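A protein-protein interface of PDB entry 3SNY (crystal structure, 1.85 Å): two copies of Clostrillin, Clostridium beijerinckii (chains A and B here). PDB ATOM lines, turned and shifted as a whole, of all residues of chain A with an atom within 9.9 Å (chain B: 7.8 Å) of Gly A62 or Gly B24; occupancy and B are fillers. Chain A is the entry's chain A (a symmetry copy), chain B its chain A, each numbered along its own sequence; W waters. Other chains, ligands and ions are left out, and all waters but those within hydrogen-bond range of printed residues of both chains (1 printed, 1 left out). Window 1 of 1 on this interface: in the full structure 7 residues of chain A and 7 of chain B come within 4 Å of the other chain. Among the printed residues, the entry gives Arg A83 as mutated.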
ATOM      1  N   ASP A  53      12.814   3.395   1.366  1.00  0.00           N
ATOM      2  CA  ASP A  53      12.255   3.536   0.025  1.00  0.00           C
ATOM      3  C   ASP A  53      13.084   4.540  -0.770  1.00  0.00           C
ATOM      4  O   ASP A  53      13.057   5.745  -0.486  1.00  0.00           O
ATOM      5  CB  ASP A  53      10.789   3.987   0.084  1.00  0.00           C
ATOM      6  CG  ASP A  53       9.851   2.896   0.588  1.00  0.00           C
ATOM      7  OD1 ASP A  53      10.105   1.696   0.340  1.00  0.00           O
ATOM      8  OD2 ASP A  53       8.839   3.245   1.226  1.00  0.00           O
ATOM      9  N   VAL A  54      13.818   4.029  -1.757  1.00  0.00           N
ATOM     10  CA  VAL A  54      14.726   4.827  -2.579  1.00  0.00           C
ATOM     11  C   VAL A  54      14.030   5.213  -3.884  1.00  0.00           C
ATOM     12  O   VAL A  54      13.565   4.342  -4.619  1.00  0.00           O
ATOM     13  CB  VAL A  54      16.032   4.037  -2.889  1.00  0.00           C
ATOM     14  CG1 VAL A  54      16.926   4.799  -3.857  1.00  0.00           C
ATOM     15  CG2 VAL A  54      16.785   3.705  -1.604  1.00  0.00           C
ATOM     16  N   TYR A  55      13.969   6.514  -4.168  1.00  0.00           N
ATOM     17  CA  TYR A  55      13.280   7.011  -5.367  1.00  0.00           C
ATOM     18  C   TYR A  55      14.230   7.542  -6.431  1.00  0.00           C
ATOM     19  O   TYR A  55      15.204   8.234  -6.129  1.00  0.00           O
ATOM     20  CB  TYR A  55      12.264   8.101  -5.015  1.00  0.00           C
ATOM     21  CG  TYR A  55      11.140   7.650  -4.111  1.00  0.00           C
ATOM     22  CD1 TYR A  55       9.920   7.222  -4.641  1.00  0.00           C
ATOM     23  CD2 TYR A  55      11.289   7.666  -2.726  1.00  0.00           C
ATOM     24  CE1 TYR A  55       8.878   6.817  -3.806  1.00  0.00           C
ATOM     25  CE2 TYR A  55      10.256   7.260  -1.886  1.00  0.00           C
ATOM     26  CZ  TYR A  55       9.059   6.837  -2.433  1.00  0.00           C
ATOM     27  OH  TYR A  55       8.042   6.444  -1.597  1.00  0.00           O
ATOM     28  N   GLU A  56      13.901   7.222  -7.679  1.00  0.00           N
ATOM     29  CA  GLU A  56      14.671   7.601  -8.860  1.00  0.00           C
ATOM     30  C   GLU A  56      14.648   9.112  -9.104  1.00  0.00           C
ATOM     31  O   GLU A  56      15.646   9.702  -9.529  1.00  0.00           O
ATOM     32  CB  GLU A  56      14.093   6.857 -10.065  1.00  0.00           C
ATOM     33  CG  GLU A  56      14.723   7.174 -11.402  1.00  0.00           C
ATOM     34  CD  GLU A  56      13.972   6.529 -12.555  1.00  0.00           C
ATOM     35  OE1 GLU A  56      12.734   6.346 -12.454  1.00  0.00           O
ATOM     36  OE2 GLU A  56      14.624   6.218 -13.570  1.00  0.00           O
ATOM     37  N   ASN A  57      13.501   9.728  -8.845  1.00  0.00           N
ATOM     38  CA  ASN A  57      13.338  11.158  -9.070  1.00  0.00           C
ATOM     39  C   ASN A  57      13.124  11.897  -7.762  1.00  0.00           C
ATOM     40  O   ASN A  57      12.913  11.276  -6.719  1.00  0.00           O
ATOM     41  CB  ASN A  57      12.179  11.415 -10.037  1.00  0.00           C
ATOM     42  CG  ASN A  57      12.440  10.846 -11.416  1.00  0.00           C
ATOM     43  OD1 ASN A  57      11.667  10.034 -11.919  1.00  0.00           O
ATOM     44  ND2 ASN A  57      13.537  11.264 -12.032  1.00  0.00           N
ATOM     45  N   ASP A  58      13.191  13.225  -7.828  1.00  0.00           N
ATOM     46  CA  ASP A  58      12.973  14.073  -6.664  1.00  0.00           C
ATOM     47  C   ASP A  58      11.521  13.969  -6.201  1.00  0.00           C
ATOM     48  O   ASP A  58      10.644  13.509  -6.952  1.00  0.00           O
ATOM     49  CB  ASP A  58      13.326  15.530  -7.001  1.00  0.00           C
ATOM     50  CG  ASP A  58      13.575  16.395  -5.760  1.00  0.00           C
ATOM     51  OD1 ASP A  58      13.458  15.901  -4.615  1.00  0.00           O
ATOM     52  OD2 ASP A  58      13.901  17.589  -5.945  1.00  0.00           O
ATOM     53  N   ASN A  59      11.290  14.371  -4.955  1.00  0.00           N
ATOM     54  CA  ASN A  59       9.946  14.476  -4.383  1.00  0.00           C
ATOM     55  C   ASN A  59       9.190  13.152  -4.361  1.00  0.00           C
ATOM     56  O   ASN A  59       7.966  13.111  -4.513  1.00  0.00           O
ATOM     57  CB  ASN A  59       9.150  15.590  -5.075  1.00  0.00           C
ATOM     58  CG  ASN A  59       9.831  16.940  -4.950  1.00  0.00           C
ATOM     59  OD1 ASN A  59      10.053  17.428  -3.841  1.00  0.00           O
ATOM     60  ND2 ASN A  59      10.175  17.542  -6.083  1.00  0.00           N
ATOM     61  N   PHE A  60       9.946  12.075  -4.155  1.00  0.00           N
ATOM     62  CA  PHE A  60       9.385  10.749  -3.899  1.00  0.00           C
ATOM     63  C   PHE A  60       8.523  10.266  -5.067  1.00  0.00           C
ATOM     64  O   PHE A  60       7.411   9.762  -4.882  1.00  0.00           O
ATOM     65  CB  PHE A  60       8.637  10.745  -2.554  1.00  0.00           C
ATOM     66  CG  PHE A  60       9.286  11.620  -1.515  1.00  0.00           C
ATOM     67  CD1 PHE A  60      10.517  11.265  -0.956  1.00  0.00           C
ATOM     68  CD2 PHE A  60       8.694  12.816  -1.124  1.00  0.00           C
ATOM     69  CE1 PHE A  60      11.135  12.081  -0.013  1.00  0.00           C
ATOM     70  CE2 PHE A  60       9.307  13.642  -0.183  1.00  0.00           C
ATOM     71  CZ  PHE A  60      10.529  13.271   0.375  1.00  0.00           C
ATOM     72  N   THR A  61       9.061  10.441  -6.275  1.00  0.00           N
ATOM     73  CA  THR A  61       8.417   9.977  -7.505  1.00  0.00           C
ATOM     74  C   THR A  61       9.404   9.197  -8.373  1.00  0.00           C
ATOM     75  O   THR A  61      10.591   9.108  -8.050  1.00  0.00           O
ATOM     76  CB  THR A  61       7.810  11.135  -8.333  1.00  0.00           C
ATOM     77  OG1 THR A  61       8.837  12.068  -8.693  1.00  0.00           O
ATOM     78  CG2 THR A  61       6.697  11.844  -7.555  1.00  0.00           C
ATOM     79  N   GLY A  62       8.903   8.644  -9.476  1.00  0.00           N
ATOM     80  CA  GLY A  62       9.674   7.732 -10.310  1.00  0.00           C
ATOM     81  C   GLY A  62       9.747   6.362  -9.666  1.00  0.00           C
ATOM     82  O   GLY A  62       9.046   6.084  -8.688  1.00  0.00           O
ATOM     83  N   THR A  63      10.603   5.502 -10.213  1.00  0.00           N
ATOM     84  CA  THR A  63      10.792   4.152  -9.684  1.00  0.00           C
ATOM     85  C   THR A  63      11.218   4.167  -8.215  1.00  0.00           C
ATOM     86  O   THR A  63      12.045   4.990  -7.800  1.00  0.00           O
ATOM     87  CB  THR A  63      11.799   3.360 -10.543  1.00  0.00           C
ATOM     88  OG1 THR A  63      11.365   3.393 -11.907  1.00  0.00           O
ATOM     89  CG2 THR A  63      11.886   1.910 -10.092  1.00  0.00           C
ATOM     90  N   LYS A  64      10.622   3.262  -7.440  1.00  0.00           N
ATOM     91  CA  LYS A  64      10.908   3.118  -6.019  1.00  0.00           C
ATOM     92  C   LYS A  64      11.513   1.748  -5.741  1.00  0.00           C
ATOM     93  O   LYS A  64      10.927   0.717  -6.089  1.00  0.00           O
ATOM     94  CB  LYS A  64       9.632   3.316  -5.196  1.00  0.00           C
ATOM     95  CG  LYS A  64       9.833   3.280  -3.683  1.00  0.00           C
ATOM     96  CD  LYS A  64       8.499   3.218  -2.945  1.00  0.00           C
ATOM     97  CE  LYS A  64       7.865   1.840  -3.065  1.00  0.00           C
ATOM     98  NZ  LYS A  64       6.413   1.859  -2.721  1.00  0.00           N
ATOM     99  N   TRP A  65      12.691   1.750  -5.121  1.00  0.00           N
ATOM    100  CA  TRP A  65      13.370   0.522  -4.707  1.00  0.00           C
ATOM    101  C   TRP A  65      13.378   0.447  -3.185  1.00  0.00           C
ATOM    102  O   TRP A  65      13.694   1.431  -2.513  1.00  0.00           O
ATOM    103  CB  TRP A  65      14.800   0.484  -5.254  1.00  0.00           C
ATOM    104  CG  TRP A  65      14.892   0.591  -6.758  1.00  0.00           C
ATOM    105  CD1 TRP A  65      14.692  -0.412  -7.667  1.00  0.00           C
ATOM    106  CD2 TRP A  65      15.227   1.761  -7.520  1.00  0.00           C
ATOM    107  NE1 TRP A  65      14.874   0.062  -8.945  1.00  0.00           N
ATOM    108  CE2 TRP A  65      15.204   1.390  -8.885  1.00  0.00           C
ATOM    109  CE3 TRP A  65      15.545   3.086  -7.183  1.00  0.00           C
ATOM    110  CZ2 TRP A  65      15.483   2.298  -9.914  1.00  0.00           C
ATOM    111  CZ3 TRP A  65      15.823   3.988  -8.207  1.00  0.00           C
ATOM    112  CH2 TRP A  65      15.789   3.587  -9.557  1.00  0.00           C
ATOM    113  N   THR A  66      13.032  -0.721  -2.647  1.00  0.00           N
ATOM    114  CA  THR A  66      12.822  -0.884  -1.209  1.00  0.00           C
ATOM    115  C   THR A  66      13.845  -1.831  -0.575  1.00  0.00           C
ATOM    116  O   THR A  66      14.088  -2.931  -1.082  1.00  0.00           O
ATOM    117  CB  THR A  66      11.380  -1.359  -0.916  1.00  0.00           C
ATOM    118  OG1 THR A  66      10.452  -0.407  -1.452  1.00  0.00           O
ATOM    119  CG2 THR A  66      11.134  -1.507   0.581  1.00  0.00           C
ATOM    120  N   LYS A  81      21.134   6.097  -8.702  1.00  0.00           N
ATOM    121  CA  LYS A  81      19.858   6.676  -9.144  1.00  0.00           C
ATOM    122  C   LYS A  81      19.120   7.470  -8.068  1.00  0.00           C
ATOM    123  O   LYS A  81      18.203   8.223  -8.390  1.00  0.00           O
ATOM    124  CB  LYS A  81      18.926   5.592  -9.714  1.00  0.00           C
ATOM    125  CG  LYS A  81      19.375   4.968 -11.046  1.00  0.00           C
ATOM    126  CD  LYS A  81      19.484   5.989 -12.180  1.00  0.00           C
ATOM    127  CE  LYS A  81      18.122   6.438 -12.704  1.00  0.00           C
ATOM    128  NZ  LYS A  81      18.210   7.712 -13.489  1.00  0.00           N
ATOM    129  N   ARG A  83      17.567  10.033  -5.836  1.00  0.00           N
ATOM    130  CA  ARG A  83      17.380  11.488  -5.790  1.00  0.00           C
ATOM    131  C   ARG A  83      16.422  11.925  -4.683  1.00  0.00           C
ATOM    132  O   ARG A  83      16.331  13.105  -4.375  1.00  0.00           O
ATOM    133  CB  ARG A  83      16.928  12.028  -7.146  1.00  0.00           C
ATOM    134  CG  ARG A  83      18.011  11.929  -8.196  1.00  0.00           C
ATOM    135  CD  ARG A  83      17.757  12.835  -9.370  1.00  0.00           C
ATOM    136  NE  ARG A  83      18.786  12.656 -10.395  1.00  0.00           N
ATOM    137  CZ  ARG A  83      18.857  13.355 -11.525  1.00  0.00           C
ATOM    138  NH1 ARG A  83      17.965  14.302 -11.793  1.00  0.00           N
ATOM    139  NH2 ARG A  83      19.832  13.105 -12.393  1.00  0.00           N
ATOM    140  N   SER A  84      15.700  10.972  -4.100  1.00  0.00           N
ATOM    141  CA  SER A  84      14.945  11.207  -2.867  1.00  0.00           C
ATOM    142  C   SER A  84      14.752   9.885  -2.138  1.00  0.00           C
ATOM    143  O   SER A  84      14.900   8.812  -2.735  1.00  0.00           O
ATOM    144  CB  SER A  84      13.607  11.921  -3.126  1.00  0.00           C
ATOM    145  OG  SER A  84      12.757  11.169  -3.968  1.00  0.00           O
ATOM    146  N   LEU B  21       6.390  -1.342 -16.109  1.00  0.00           N
ATOM    147  CA  LEU B  21       6.937  -0.472 -15.069  1.00  0.00           C
ATOM    148  C   LEU B  21       7.196  -1.210 -13.765  1.00  0.00           C
ATOM    149  O   LEU B  21       6.429  -2.090 -13.366  1.00  0.00           O
ATOM    150  CB  LEU B  21       6.002   0.712 -14.793  1.00  0.00           C
ATOM    151  CG  LEU B  21       5.849   1.829 -15.827  1.00  0.00           C
ATOM    152  CD1 LEU B  21       4.888   2.889 -15.289  1.00  0.00           C
ATOM    153  CD2 LEU B  21       7.200   2.457 -16.183  1.00  0.00           C
ATOM    154  N   GLN B  22       8.285  -0.829 -13.104  1.00  0.00           N
ATOM    155  CA  GLN B  22       8.629  -1.325 -11.783  1.00  0.00           C
ATOM    156  C   GLN B  22       7.854  -0.535 -10.725  1.00  0.00           C
ATOM    157  O   GLN B  22       7.239   0.478 -11.059  1.00  0.00           O
ATOM    158  CB  GLN B  22      10.141  -1.192 -11.565  1.00  0.00           C
ATOM    159  CG  GLN B  22      10.971  -2.192 -12.370  1.00  0.00           C
ATOM    160  CD  GLN B  22      10.615  -3.635 -12.052  1.00  0.00           C
ATOM    161  OE1 GLN B  22      10.734  -4.082 -10.910  1.00  0.00           O
ATOM    162  NE2 GLN B  22      10.169  -4.371 -13.066  1.00  0.00           N
ATOM    163  N   PRO B  23       7.866  -0.994  -9.452  1.00  0.00           N
ATOM    164  CA  PRO B  23       7.222  -0.220  -8.390  1.00  0.00           C
ATOM    165  C   PRO B  23       7.699   1.230  -8.381  1.00  0.00           C
ATOM    166  O   PRO B  23       8.848   1.506  -8.729  1.00  0.00           O
ATOM    167  CB  PRO B  23       7.681  -0.927  -7.116  1.00  0.00           C
ATOM    168  CG  PRO B  23       7.874  -2.336  -7.539  1.00  0.00           C
ATOM    169  CD  PRO B  23       8.439  -2.250  -8.930  1.00  0.00           C
ATOM    170  N   GLY B  24       6.811   2.137  -7.999  1.00  0.00           N
ATOM    171  CA  GLY B  24       7.139   3.554  -7.959  1.00  0.00           C
ATOM    172  C   GLY B  24       5.911   4.430  -8.065  1.00  0.00           C
ATOM    173  O   GLY B  24       4.791   3.936  -8.218  1.00  0.00           O
ATOM    174  N   ASN B  25       6.132   5.738  -7.978  1.00  0.00           N
ATOM    175  CA  ASN B  25       5.053   6.716  -8.043  1.00  0.00           C
ATOM    176  C   ASN B  25       5.289   7.589  -9.259  1.00  0.00           C
ATOM    177  O   ASN B  25       6.180   8.439  -9.259  1.00  0.00           O
ATOM    178  CB  ASN B  25       5.019   7.563  -6.764  1.00  0.00           C
ATOM    179  CG  ASN B  25       4.969   6.722  -5.500  1.00  0.00           C
ATOM    180  OD1 ASN B  25       4.385   5.634  -5.480  1.00  0.00           O
ATOM    181  ND2 ASN B  25       5.585   7.227  -4.431  1.00  0.00           N
ATOM    182  N   TYR B  26       4.505   7.360 -10.304  1.00  0.00           N
ATOM    183  CA  TYR B  26       4.759   7.990 -11.592  1.00  0.00           C
ATOM    184  C   TYR B  26       3.744   9.077 -11.905  1.00  0.00           C
ATOM    185  O   TYR B  26       2.539   8.818 -11.973  1.00  0.00           O
ATOM    186  CB  TYR B  26       4.782   6.937 -12.705  1.00  0.00           C
ATOM    187  CG  TYR B  26       5.776   5.820 -12.473  1.00  0.00           C
ATOM    188  CD1 TYR B  26       7.087   5.923 -12.936  1.00  0.00           C
ATOM    189  CD2 TYR B  26       5.403   4.658 -11.798  1.00  0.00           C
ATOM    190  CE1 TYR B  26       8.002   4.892 -12.734  1.00  0.00           C
ATOM    191  CE2 TYR B  26       6.309   3.622 -11.589  1.00  0.00           C
ATOM    192  CZ  TYR B  26       7.605   3.748 -12.057  1.00  0.00           C
ATOM    193  OH  TYR B  26       8.499   2.727 -11.854  1.00  0.00           O
ATOM    194  N   THR B  27       4.246  10.298 -12.080  1.00  0.00           N
ATOM    195  CA  THR B  27       3.430  11.434 -12.500  1.00  0.00           C
ATOM    196  C   THR B  27       3.120  11.313 -13.995  1.00  0.00           C
ATOM    197  O   THR B  27       3.679  10.449 -14.683  1.00  0.00           O
ATOM    198  CB  THR B  27       4.166  12.772 -12.256  1.00  0.00           C
ATOM    199  OG1 THR B  27       5.338  12.820 -13.081  1.00  0.00           O
ATOM    200  CG2 THR B  27       4.568  12.918 -10.789  1.00  0.00           C
ATOM    201  N   GLN B  30       6.211  11.721 -16.134  1.00  0.00           N
ATOM    202  CA  GLN B  30       7.055  10.537 -15.990  1.00  0.00           C
ATOM    203  C   GLN B  30       6.502   9.348 -16.781  1.00  0.00           C
ATOM    204  O   GLN B  30       7.262   8.603 -17.412  1.00  0.00           O
ATOM    205  CB  GLN B  30       7.233  10.192 -14.512  1.00  0.00           C
ATOM    206  CG  GLN B  30       8.139  11.175 -13.777  1.00  0.00           C
ATOM    207  CD  GLN B  30       8.040  11.082 -12.262  1.00  0.00           C
ATOM    208  OE1 GLN B  30       7.186  10.380 -11.713  1.00  0.00           O
ATOM    209  NE2 GLN B  30       8.918  11.808 -11.575  1.00  0.00           N
ATOM    210  N   TRP B  50       1.141  -7.741  -5.636  1.00  0.00           N
ATOM    211  CA  TRP B  50       1.357  -6.327  -5.956  1.00  0.00           C
ATOM    212  C   TRP B  50       0.047  -5.530  -5.964  1.00  0.00           C
ATOM    213  O   TRP B  50      -1.045  -6.102  -6.075  1.00  0.00           O
ATOM    214  CB  TRP B  50       2.057  -6.186  -7.313  1.00  0.00           C
ATOM    215  CG  TRP B  50       3.511  -6.604  -7.351  1.00  0.00           C
ATOM    216  CD1 TRP B  50       4.109  -7.601  -6.625  1.00  0.00           C
ATOM    217  CD2 TRP B  50       4.533  -6.058  -8.194  1.00  0.00           C
ATOM    218  NE1 TRP B  50       5.441  -7.693  -6.952  1.00  0.00           N
ATOM    219  CE2 TRP B  50       5.727  -6.762  -7.916  1.00  0.00           C
ATOM    220  CE3 TRP B  50       4.557  -5.037  -9.155  1.00  0.00           C
ATOM    221  CZ2 TRP B  50       6.936  -6.474  -8.561  1.00  0.00           C
ATOM    222  CZ3 TRP B  50       5.761  -4.753  -9.801  1.00  0.00           C
ATOM    223  CH2 TRP B  50       6.933  -5.474  -9.500  1.00  0.00           C
ATOM    224  N   THR B  51       0.168  -4.207  -5.843  1.00  0.00           N
ATOM    225  CA  THR B  51      -0.976  -3.296  -5.878  1.00  0.00           C
ATOM    226  C   THR B  51      -0.707  -2.156  -6.857  1.00  0.00           C
ATOM    227  O   THR B  51       0.380  -1.576  -6.861  1.00  0.00           O
ATOM    228  CB  THR B  51      -1.281  -2.707  -4.480  1.00  0.00           C
ATOM    229  OG1 THR B  51      -1.520  -3.771  -3.553  1.00  0.00           O
ATOM    230  CG2 THR B  51      -2.507  -1.794  -4.516  1.00  0.00           C
ATOM    231  N   ASP B  53      -2.409   1.447  -7.944  1.00  0.00           N
ATOM    232  CA  ASP B  53      -3.380   2.520  -7.748  1.00  0.00           C
ATOM    233  C   ASP B  53      -3.339   3.468  -8.942  1.00  0.00           C
ATOM    234  O   ASP B  53      -2.361   4.206  -9.129  1.00  0.00           O
ATOM    235  CB  ASP B  53      -3.098   3.288  -6.450  1.00  0.00           C
ATOM    236  CG  ASP B  53      -3.423   2.480  -5.199  1.00  0.00           C
ATOM    237  OD1 ASP B  53      -4.361   1.653  -5.221  1.00  0.00           O
ATOM    238  OD2 ASP B  53      -2.740   2.687  -4.176  1.00  0.00           O
ATOM    239  N   PHE B  60      -1.332  12.060  -8.456  1.00  0.00           N
ATOM    240  CA  PHE B  60      -1.985  11.103  -7.563  1.00  0.00           C
ATOM    241  C   PHE B  60      -3.224  11.707  -6.899  1.00  0.00           C
ATOM    242  O   PHE B  60      -3.432  11.579  -5.688  1.00  0.00           O
ATOM    243  CB  PHE B  60      -0.966  10.548  -6.552  1.00  0.00           C
ATOM    244  CG  PHE B  60       0.412  10.379  -7.134  1.00  0.00           C
ATOM    245  CD1 PHE B  60       0.663   9.395  -8.093  1.00  0.00           C
ATOM    246  CD2 PHE B  60       1.449  11.228  -6.759  1.00  0.00           C
ATOM    247  CE1 PHE B  60       1.928   9.249  -8.653  1.00  0.00           C
ATOM    248  CE2 PHE B  60       2.719  11.092  -7.317  1.00  0.00           C
ATOM    249  CZ  PHE B  60       2.958  10.098  -8.264  1.00  0.00           C
ATOM    250  N   VAL B  85       0.053   7.106 -11.493  1.00  0.00           N
ATOM    251  CA  VAL B  85      -0.063   5.750 -10.967  1.00  0.00           C
ATOM    252  C   VAL B  85       0.950   5.488  -9.857  1.00  0.00           C
ATOM    253  O   VAL B  85       2.097   5.945  -9.924  1.00  0.00           O
ATOM    254  CB  VAL B  85       0.045   4.684 -12.112  1.00  0.00           C
ATOM    255  CG1 VAL B  85       1.441   4.660 -12.735  1.00  0.00           C
ATOM    256  CG2 VAL B  85      -0.365   3.292 -11.626  1.00  0.00           C
ATOM    257  N   LYS B  86       0.508   4.771  -8.828  1.00  0.00           N
ATOM    258  CA  LYS B  86       1.412   4.254  -7.808  1.00  0.00           C
ATOM    259  C   LYS B  86       1.414   2.733  -7.870  1.00  0.00           C
ATOM    260  O   LYS B  86       0.354   2.104  -7.876  1.00  0.00           O
ATOM    261  CB  LYS B  86       1.012   4.740  -6.417  1.00  0.00           C
ATOM    262  CG  LYS B  86       1.166   6.243  -6.223  1.00  0.00           C
ATOM    263  CD  LYS B  86       0.945   6.613  -4.768  1.00  0.00           C
ATOM    264  CE  LYS B  86       1.095   8.102  -4.533  1.00  0.00           C
ATOM    265  NZ  LYS B  86       1.056   8.424  -3.076  1.00  0.00           N
ATOM    266  N   ILE B  87       2.612   2.159  -7.942  1.00  0.00           N
ATOM    267  CA  ILE B  87       2.786   0.710  -8.029  1.00  0.00           C
ATOM    268  C   ILE B  87       3.553   0.225  -6.799  1.00  0.00           C
ATOM    269  O   ILE B  87       4.605   0.767  -6.469  1.00  0.00           O
ATOM    270  CB  ILE B  87       3.544   0.302  -9.325  1.00  0.00           C
ATOM    271  CG1 ILE B  87       2.776   0.758 -10.573  1.00  0.00           C
ATOM    272  CG2 ILE B  87       3.783  -1.212  -9.366  1.00  0.00           C
ATOM    273  CD1 ILE B  87       3.605   0.772 -11.851  1.00  0.00           C
ATOM    274  N   TYR B  88       3.006  -0.783  -6.123  1.00  0.00           N
ATOM    275  CA  TYR B  88       3.631  -1.370  -4.938  1.00  0.00           C
ATOM    276  C   TYR B  88       3.860  -2.859  -5.143  1.00  0.00           C
ATOM    277  O   TYR B  88       3.024  -3.540  -5.737  1.00  0.00           O
ATOM    278  CB  TYR B  88       2.735  -1.189  -3.711  1.00  0.00           C
ATOM    279  CG  TYR B  88       2.359   0.239  -3.398  1.00  0.00           C
ATOM    280  CD1 TYR B  88       3.126   1.002  -2.517  1.00  0.00           C
ATOM    281  CD2 TYR B  88       1.226   0.824  -3.967  1.00  0.00           C
ATOM    282  CE1 TYR B  88       2.782   2.313  -2.217  1.00  0.00           C
ATOM    283  CE2 TYR B  88       0.872   2.134  -3.673  1.00  0.00           C
ATOM    284  CZ  TYR B  88       1.657   2.871  -2.799  1.00  0.00           C
ATOM    285  OH  TYR B  88       1.314   4.167  -2.504  1.00  0.00           O
ATOM    286  N   SER B  89       4.985  -3.363  -4.641  1.00  0.00           N
ATOM    287  CA  SER B  89       5.230  -4.808  -4.621  1.00  0.00           C
ATOM    288  C   SER B  89       4.643  -5.458  -3.355  1.00  0.00           C
ATOM    289  O   SER B  89       4.975  -6.603  -3.020  1.00  0.00           O
ATOM    290  CB  SER B  89       6.726  -5.113  -4.769  1.00  0.00           C
ATOM    291  OG  SER B  89       7.468  -4.552  -3.704  1.00  0.00           O
HETATM  292  O   HOH W   1       6.843  -1.297  -3.465  1.00  0.00           O
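Asn A59 touches none of the printed residues of chain B. Gly A62 touches four residues of chain B. Of the printed residues of chain B, Thr A63 touches Gln B22, Pro B23 and Tyr B26. Of chain A, only Thr A63 and Lys A64 come within 4 Å of Pro B23. Gly B24 touches two residues of chain A. Printed residues of chain A within 4 Å of Tyr B26: Gly A62 (3.8 Å) and Thr A63 (2.9 Å). No residue of chain A comes within 4 Å of Ile B87. The nearest residue of chain B that does not touch Gly A62 is Pro B23 (4.6 Å).
Positions printed for both chains: 53 and 60. Of the 15 pairs that touch across the chains among the printed residues, none has its exchanged pair printed and touching as well.
Of the 17 printed residues of chain A, 7 touch a printed residue of chain B. Printed residues of chain A that touch a printed residue of chain B: Tyr A55, Asn A57, Phe A60, Thr A61, Gly A62, Thr A63 and Lys A64. Among the printed residues, 15 pairs touch across the chains. Among the printed residues, no Asp or Glu carboxylate lies within 4 Å of a Lys or Arg side-chain nitrogen of the other chain.
The backbone carbonyl oxygen (O) of Pro B23 is in hydrogen-bond range of the backbone NH (N) of Lys A64, 2.8 Å away. The backbone carbonyl oxygen (O) of Phe A60 sits at hydrogen-bond distance from the side-chain amide nitrogen (ND2) of Asn B25, at 3.2 Å. O of Asn B25 lies within hydrogen-bond range of N of Gly A62 (2.7 Å). OH of Tyr B26 lies within hydrogen-bond range of OG1 of Thr A63 (2.9 Å). The side-chain amide oxygen (OD1) of Asn A57 is in hydrogen-bond range of the side-chain amide nitrogen (NE2) of Gln B30 (3.3 Å). The side-chain hydroxyl (OG1) of Thr A61 sits at hydrogen-bond distance from the side-chain amide nitrogen (NE2) of Gln B30 (2.9 Å). OE1 of Gln B30 is in hydrogen-bond range of N of Gly A62.
Asn B25 touches Tyr A55. Asn B25 touches Thr A61. Gly A62 touches Gly B24 (O to CA, 3.3 Å). CE1 of Tyr B26 touches C of Gly A62 (3.8 Å). Thr A63 touches Gln B22 (CG2 to CB, 3.9 Å). O of Pro B23 touches CG2 of Thr A63, at 3.4 Å. Lys A64 touches Gly B24. NZ of Lys A64 touches CD1 of Tyr B88, at 3.4 Å.
Water W1 bridges N of Ser B89 and NZ of Lys A64.
O of Gln B22 is in hydrogen-bond range of OH of Tyr B26, at 2.7 Å. The backbone carbonyl oxygen (O) of Asn B25 lies close to the side-chain amide oxygen (OE1) of Gln B30 (3.3 Å). N of Thr B27 is in hydrogen-bond range of OE1 of Gln B30, at 3.0 Å. O of Thr B51 is in hydrogen-bond range of N of Tyr B88 (2.8 Å). The side-chain hydroxyl (OG) of Ser A84 sits at hydrogen-bond distance from the backbone carbonyl oxygen (O) of Asn A57, 2.8 Å away. The backbone NH (N) of Phe A60 is in hydrogen-bond range of the side-chain hydroxyl (OG) of Ser A84.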
